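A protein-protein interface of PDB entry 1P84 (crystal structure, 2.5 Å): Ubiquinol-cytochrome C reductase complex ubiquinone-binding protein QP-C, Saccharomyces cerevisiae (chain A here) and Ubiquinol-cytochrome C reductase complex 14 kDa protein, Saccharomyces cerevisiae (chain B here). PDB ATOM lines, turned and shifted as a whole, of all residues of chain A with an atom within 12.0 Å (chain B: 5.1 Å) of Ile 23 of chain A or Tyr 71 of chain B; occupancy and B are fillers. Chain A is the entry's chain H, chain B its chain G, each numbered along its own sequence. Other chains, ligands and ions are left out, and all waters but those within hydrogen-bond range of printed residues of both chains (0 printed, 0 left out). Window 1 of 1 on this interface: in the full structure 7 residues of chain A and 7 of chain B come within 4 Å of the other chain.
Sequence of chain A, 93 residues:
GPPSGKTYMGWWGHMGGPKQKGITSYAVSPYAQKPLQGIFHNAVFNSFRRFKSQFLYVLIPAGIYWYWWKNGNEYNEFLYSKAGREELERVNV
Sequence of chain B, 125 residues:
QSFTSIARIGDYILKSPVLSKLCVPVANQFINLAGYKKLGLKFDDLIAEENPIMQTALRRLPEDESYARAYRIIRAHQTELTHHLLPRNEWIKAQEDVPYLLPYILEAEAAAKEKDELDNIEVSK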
ATOM      1  N   GLY A  17       2.162  22.734  12.328  1.00  0.00           N
ATOM      2  CA  GLY A  17       0.967  22.025  11.910  1.00  0.00           C
ATOM      3  C   GLY A  17       1.166  21.333  10.579  1.00  0.00           C
ATOM      4  O   GLY A  17       2.251  21.394  10.007  1.00  0.00           O
ATOM      5  N   PRO A  18       0.144  20.645  10.064  1.00  0.00           N
ATOM      6  CA  PRO A  18       0.269  19.957   8.780  1.00  0.00           C
ATOM      7  C   PRO A  18       0.069  20.954   7.630  1.00  0.00           C
ATOM      8  O   PRO A  18      -0.539  22.015   7.818  1.00  0.00           O
ATOM      9  CB  PRO A  18      -0.868  18.946   8.848  1.00  0.00           C
ATOM     10  CG  PRO A  18      -1.941  19.736   9.528  1.00  0.00           C
ATOM     11  CD  PRO A  18      -1.180  20.399  10.663  1.00  0.00           C
ATOM     12  N   LYS A  19       0.569  20.611   6.445  1.00  0.00           N
ATOM     13  CA  LYS A  19       0.425  21.494   5.294  1.00  0.00           C
ATOM     14  C   LYS A  19      -1.039  21.689   4.941  1.00  0.00           C
ATOM     15  O   LYS A  19      -1.767  20.726   4.740  1.00  0.00           O
ATOM     16  CB  LYS A  19       1.204  20.957   4.098  1.00  0.00           C
ATOM     17  CG  LYS A  19       2.685  20.818   4.365  1.00  0.00           C
ATOM     18  CD  LYS A  19       3.474  20.639   3.081  1.00  0.00           C
ATOM     19  CE  LYS A  19       4.855  20.047   3.361  1.00  0.00           C
ATOM     20  NZ  LYS A  19       5.552  20.763   4.480  1.00  0.00           N
ATOM     21  N   GLN A  20      -1.474  22.940   4.925  1.00  0.00           N
ATOM     22  CA  GLN A  20      -2.857  23.275   4.618  1.00  0.00           C
ATOM     23  C   GLN A  20      -3.017  23.612   3.145  1.00  0.00           C
ATOM     24  O   GLN A  20      -2.138  24.210   2.548  1.00  0.00           O
ATOM     25  CB  GLN A  20      -3.307  24.460   5.473  1.00  0.00           C
ATOM     26  CG  GLN A  20      -3.162  24.250   6.971  1.00  0.00           C
ATOM     27  CD  GLN A  20      -3.734  25.403   7.771  1.00  0.00           C
ATOM     28  OE1 GLN A  20      -4.557  26.174   7.268  1.00  0.00           O
ATOM     29  NE2 GLN A  20      -3.302  25.532   9.024  1.00  0.00           N
ATOM     30  N   LYS A  21      -4.161  23.253   2.577  1.00  0.00           N
ATOM     31  CA  LYS A  21      -4.466  23.492   1.167  1.00  0.00           C
ATOM     32  C   LYS A  21      -5.978  23.319   1.010  1.00  0.00           C
ATOM     33  O   LYS A  21      -6.589  22.530   1.726  1.00  0.00           O
ATOM     34  CB  LYS A  21      -3.738  22.449   0.306  1.00  0.00           C
ATOM     35  CG  LYS A  21      -3.596  22.785  -1.174  1.00  0.00           C
ATOM     36  CD  LYS A  21      -2.986  21.597  -1.939  1.00  0.00           C
ATOM     37  CE  LYS A  21      -2.416  21.979  -3.312  1.00  0.00           C
ATOM     38  NZ  LYS A  21      -3.390  22.717  -4.173  1.00  0.00           N
ATOM     39  N   GLY A  22      -6.584  24.094   0.122  1.00  0.00           N
ATOM     40  CA  GLY A  22      -8.013  23.978  -0.108  1.00  0.00           C
ATOM     41  C   GLY A  22      -8.921  24.812   0.774  1.00  0.00           C
ATOM     42  O   GLY A  22     -10.086  25.038   0.423  1.00  0.00           O
ATOM     43  N   ILE A  23      -8.411  25.245   1.927  1.00  0.00           N
ATOM     44  CA  ILE A  23      -9.191  26.060   2.862  1.00  0.00           C
ATOM     45  C   ILE A  23      -9.031  27.550   2.551  1.00  0.00           C
ATOM     46  O   ILE A  23      -7.915  28.042   2.399  1.00  0.00           O
ATOM     47  CB  ILE A  23      -8.748  25.808   4.312  1.00  0.00           C
ATOM     48  CG1 ILE A  23      -8.800  24.312   4.615  1.00  0.00           C
ATOM     49  CG2 ILE A  23      -9.647  26.574   5.276  1.00  0.00           C
ATOM     50  CD1 ILE A  23      -7.826  23.878   5.682  1.00  0.00           C
ATOM     51  N   THR A  24     -10.150  28.264   2.511  1.00  0.00           N
ATOM     52  CA  THR A  24     -10.154  29.686   2.211  1.00  0.00           C
ATOM     53  C   THR A  24     -10.934  30.477   3.264  1.00  0.00           C
ATOM     54  O   THR A  24     -12.117  30.234   3.476  1.00  0.00           O
ATOM     55  CB  THR A  24     -10.777  29.925   0.805  1.00  0.00           C
ATOM     56  OG1 THR A  24      -9.942  29.319  -0.187  1.00  0.00           O
ATOM     57  CG2 THR A  24     -10.923  31.418   0.498  1.00  0.00           C
ATOM     58  N   SER A  25     -10.279  31.439   3.909  1.00  0.00           N
ATOM     59  CA  SER A  25     -10.944  32.239   4.935  1.00  0.00           C
ATOM     60  C   SER A  25     -11.307  33.614   4.420  1.00  0.00           C
ATOM     61  O   SER A  25     -10.659  34.132   3.513  1.00  0.00           O
ATOM     62  CB  SER A  25     -10.086  32.346   6.210  1.00  0.00           C
ATOM     63  OG  SER A  25      -8.801  32.907   5.967  1.00  0.00           O
ATOM     64  N   TYR A  26     -12.366  34.176   4.993  1.00  0.00           N
ATOM     65  CA  TYR A  26     -12.867  35.495   4.627  1.00  0.00           C
ATOM     66  C   TYR A  26     -13.197  36.267   5.893  1.00  0.00           C
ATOM     67  O   TYR A  26     -13.707  35.692   6.858  1.00  0.00           O
ATOM     68  CB  TYR A  26     -14.169  35.382   3.829  1.00  0.00           C
ATOM     69  CG  TYR A  26     -14.077  34.674   2.498  1.00  0.00           C
ATOM     70  CD1 TYR A  26     -14.120  33.282   2.419  1.00  0.00           C
ATOM     71  CD2 TYR A  26     -14.029  35.399   1.304  1.00  0.00           C
ATOM     72  CE1 TYR A  26     -14.124  32.634   1.185  1.00  0.00           C
ATOM     73  CE2 TYR A  26     -14.037  34.756   0.067  1.00  0.00           C
ATOM     74  CZ  TYR A  26     -14.087  33.379   0.015  1.00  0.00           C
ATOM     75  OH  TYR A  26     -14.120  32.748  -1.207  1.00  0.00           O
ATOM     76  N   ALA A  27     -12.969  37.575   5.874  1.00  0.00           N
ATOM     77  CA  ALA A  27     -13.282  38.400   7.031  1.00  0.00           C
ATOM     78  C   ALA A  27     -13.591  39.823   6.608  1.00  0.00           C
ATOM     79  O   ALA A  27     -13.190  40.262   5.538  1.00  0.00           O
ATOM     80  CB  ALA A  27     -12.135  38.375   8.043  1.00  0.00           C
ATOM     81  N   TYR B  67      -5.737  16.935   4.535  1.00  0.00           N
ATOM     82  CA  TYR B  67      -6.314  18.251   4.265  1.00  0.00           C
ATOM     83  C   TYR B  67      -7.685  18.345   4.919  1.00  0.00           C
ATOM     84  O   TYR B  67      -8.071  19.400   5.433  1.00  0.00           O
ATOM     85  CB  TYR B  67      -6.454  18.509   2.758  1.00  0.00           C
ATOM     86  CG  TYR B  67      -5.148  18.593   1.989  1.00  0.00           C
ATOM     87  CD1 TYR B  67      -5.037  18.040   0.714  1.00  0.00           C
ATOM     88  CD2 TYR B  67      -4.023  19.220   2.534  1.00  0.00           C
ATOM     89  CE1 TYR B  67      -3.849  18.106   0.006  1.00  0.00           C
ATOM     90  CE2 TYR B  67      -2.825  19.290   1.830  1.00  0.00           C
ATOM     91  CZ  TYR B  67      -2.747  18.730   0.568  1.00  0.00           C
ATOM     92  OH  TYR B  67      -1.569  18.786  -0.141  1.00  0.00           O
ATOM     93  N   ALA B  68      -8.424  17.235   4.882  1.00  0.00           N
ATOM     94  CA  ALA B  68      -9.753  17.168   5.487  1.00  0.00           C
ATOM     95  C   ALA B  68      -9.691  17.297   7.027  1.00  0.00           C
ATOM     96  O   ALA B  68     -10.493  18.025   7.629  1.00  0.00           O
ATOM     97  CB  ALA B  68     -10.434  15.880   5.090  1.00  0.00           C
ATOM     98  N   ARG B  69      -8.735  16.612   7.658  1.00  0.00           N
ATOM     99  CA  ARG B  69      -8.598  16.691   9.108  1.00  0.00           C
ATOM    100  C   ARG B  69      -8.344  18.146   9.484  1.00  0.00           C
ATOM    101  O   ARG B  69      -8.946  18.669  10.435  1.00  0.00           O
ATOM    102  CB  ARG B  69      -7.450  15.819   9.625  1.00  0.00           C
ATOM    103  CG  ARG B  69      -7.502  15.620  11.141  1.00  0.00           C
ATOM    104  CD  ARG B  69      -6.297  14.877  11.713  1.00  0.00           C
ATOM    105  NE  ARG B  69      -5.123  15.729  11.689  1.00  0.00           N
ATOM    106  CZ  ARG B  69      -4.426  16.099  12.753  1.00  0.00           C
ATOM    107  NH1 ARG B  69      -3.380  16.893  12.587  1.00  0.00           N
ATOM    108  NH2 ARG B  69      -4.744  15.670  13.964  1.00  0.00           N
ATOM    109  N   ALA B  70      -7.501  18.807   8.685  1.00  0.00           N
ATOM    110  CA  ALA B  70      -7.143  20.202   8.904  1.00  0.00           C
ATOM    111  C   ALA B  70      -8.365  21.104   8.859  1.00  0.00           C
ATOM    112  O   ALA B  70      -8.551  21.951   9.737  1.00  0.00           O
ATOM    113  CB  ALA B  70      -6.123  20.650   7.875  1.00  0.00           C
ATOM    114  N   TYR B  71      -9.214  20.905   7.854  1.00  0.00           N
ATOM    115  CA  TYR B  71     -10.416  21.725   7.734  1.00  0.00           C
ATOM    116  C   TYR B  71     -11.376  21.491   8.893  1.00  0.00           C
ATOM    117  O   TYR B  71     -12.025  22.425   9.377  1.00  0.00           O
ATOM    118  CB  TYR B  71     -11.147  21.472   6.404  1.00  0.00           C
ATOM    119  CG  TYR B  71     -12.465  22.222   6.300  1.00  0.00           C
ATOM    120  CD1 TYR B  71     -12.513  23.607   6.446  1.00  0.00           C
ATOM    121  CD2 TYR B  71     -13.667  21.541   6.110  1.00  0.00           C
ATOM    122  CE1 TYR B  71     -13.721  24.300   6.407  1.00  0.00           C
ATOM    123  CE2 TYR B  71     -14.887  22.224   6.072  1.00  0.00           C
ATOM    124  CZ  TYR B  71     -14.905  23.604   6.219  1.00  0.00           C
ATOM    125  OH  TYR B  71     -16.101  24.285   6.163  1.00  0.00           O
ATOM    126  N   ARG B  72     -11.486  20.242   9.325  1.00  0.00           N
ATOM    127  CA  ARG B  72     -12.394  19.933  10.414  1.00  0.00           C
ATOM    128  C   ARG B  72     -11.950  20.578  11.715  1.00  0.00           C
ATOM    129  O   ARG B  72     -12.762  21.185  12.419  1.00  0.00           O
ATOM    130  CB  ARG B  72     -12.573  18.419  10.570  1.00  0.00           C
ATOM    131  CG  ARG B  72     -13.393  17.790   9.434  1.00  0.00           C
ATOM    132  CD  ARG B  72     -13.875  16.405   9.786  1.00  0.00           C
ATOM    133  NE  ARG B  72     -12.779  15.486  10.074  1.00  0.00           N
ATOM    134  CZ  ARG B  72     -12.161  14.749   9.161  1.00  0.00           C
ATOM    135  NH1 ARG B  72     -11.177  13.936   9.525  1.00  0.00           N
ATOM    136  NH2 ARG B  72     -12.527  14.823   7.886  1.00  0.00           N
ATOM    137  N   ILE B  73     -10.652  20.511  11.992  1.00  0.00           N
ATOM    138  CA  ILE B  73     -10.110  21.093  13.215  1.00  0.00           C
ATOM    139  C   ILE B  73     -10.254  22.622  13.278  1.00  0.00           C
ATOM    140  O   ILE B  73     -10.685  23.167  14.300  1.00  0.00           O
ATOM    141  CB  ILE B  73      -8.656  20.640  13.431  1.00  0.00           C
ATOM    142  CG1 ILE B  73      -8.648  19.133  13.743  1.00  0.00           C
ATOM    143  CG2 ILE B  73      -8.000  21.451  14.539  1.00  0.00           C
ATOM    144  CD1 ILE B  73      -7.269  18.501  13.785  1.00  0.00           C
ATOM    145  N   ILE B  74      -9.946  23.300  12.175  1.00  0.00           N
ATOM    146  CA  ILE B  74     -10.067  24.755  12.117  1.00  0.00           C
ATOM    147  C   ILE B  74     -11.529  25.174  12.288  1.00  0.00           C
ATOM    148  O   ILE B  74     -11.845  26.076  13.087  1.00  0.00           O
ATOM    149  CB  ILE B  74      -9.514  25.319  10.787  1.00  0.00           C
ATOM    150  CG1 ILE B  74      -8.028  24.979  10.655  1.00  0.00           C
ATOM    151  CG2 ILE B  74      -9.701  26.832  10.728  1.00  0.00           C
ATOM    152  CD1 ILE B  74      -7.419  25.381   9.335  1.00  0.00           C
ATOM    153  N   ARG B  75     -12.413  24.491  11.560  1.00  0.00           N
ATOM    154  CA  ARG B  75     -13.854  24.749  11.608  1.00  0.00           C
ATOM    155  C   ARG B  75     -14.385  24.589  13.039  1.00  0.00           C
ATOM    156  O   ARG B  75     -15.237  25.358  13.490  1.00  0.00           O
ATOM    157  CB  ARG B  75     -14.576  23.780  10.667  1.00  0.00           C
ATOM    158  CG  ARG B  75     -16.097  23.938  10.585  1.00  0.00           C
ATOM    159  CD  ARG B  75     -16.778  22.574  10.654  1.00  0.00           C
ATOM    160  NE  ARG B  75     -17.277  22.087   9.373  1.00  0.00           N
ATOM    161  CZ  ARG B  75     -17.257  20.810   8.993  1.00  0.00           C
ATOM    162  NH1 ARG B  75     -17.752  20.474   7.809  1.00  0.00           N
ATOM    163  NH2 ARG B  75     -16.709  19.876   9.762  1.00  0.00           N
ATOM    164  N   ALA B  76     -13.842  23.610  13.758  1.00  0.00           N
ATOM    165  CA  ALA B  76     -14.246  23.346  15.136  1.00  0.00           C
ATOM    166  C   ALA B  76     -13.864  24.496  16.069  1.00  0.00           C
ATOM    167  O   ALA B  76     -14.683  24.947  16.877  1.00  0.00           O
ATOM    168  CB  ALA B  76     -13.628  22.037  15.623  1.00  0.00           C
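Among the printed residues, pairs that only touch across the chains: Lys 19 of chain A with Tyr 67 of chain B (3.4 Å), Gln 20 of chain A with Ile 74 of chain B (3.6 Å), Lys 21 of chain A with Tyr 67 of chain B (3.6 Å), Ile 23 of chain A with Tyr 71 of chain B (3.9 Å) and Ile 23 of chain A with Ile 74 of chain B (3.97 Å).
Tyr 71 of chain B touches just one residue of chain A: Ile 23 (3.9 Å). No residue of chain A comes within 4 Å of Ala 70 of chain B. No residue of chain A comes within 4 Å of Arg 72 of chain B. Of the printed residues of chain A, Ile 74 of chain B touches Gln 20 and Ile 23. Of the printed residues of chain B, Lys 21 of chain A touches Tyr 67. Printed residues of chain B within 4 Å of Gln 20 of chain A: Ile 74 (3.6 Å). Printed residues of chain A within 4 Å of Tyr 67 of chain B: Lys 19 and Lys 21. Ala 76 of chain B touches none of the printed residues of chain A.
Hydrophobic or aromatic side chains of chain A within 4 Å of the printed part of chain B: Ile 23. Of the 10 printed residues of chain B, 3 touch a printed residue of chain A. Among the printed residues, no Asp or Glu carboxylate lies within 4 Å of a Lys or Arg side-chain nitrogen of the other chain.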
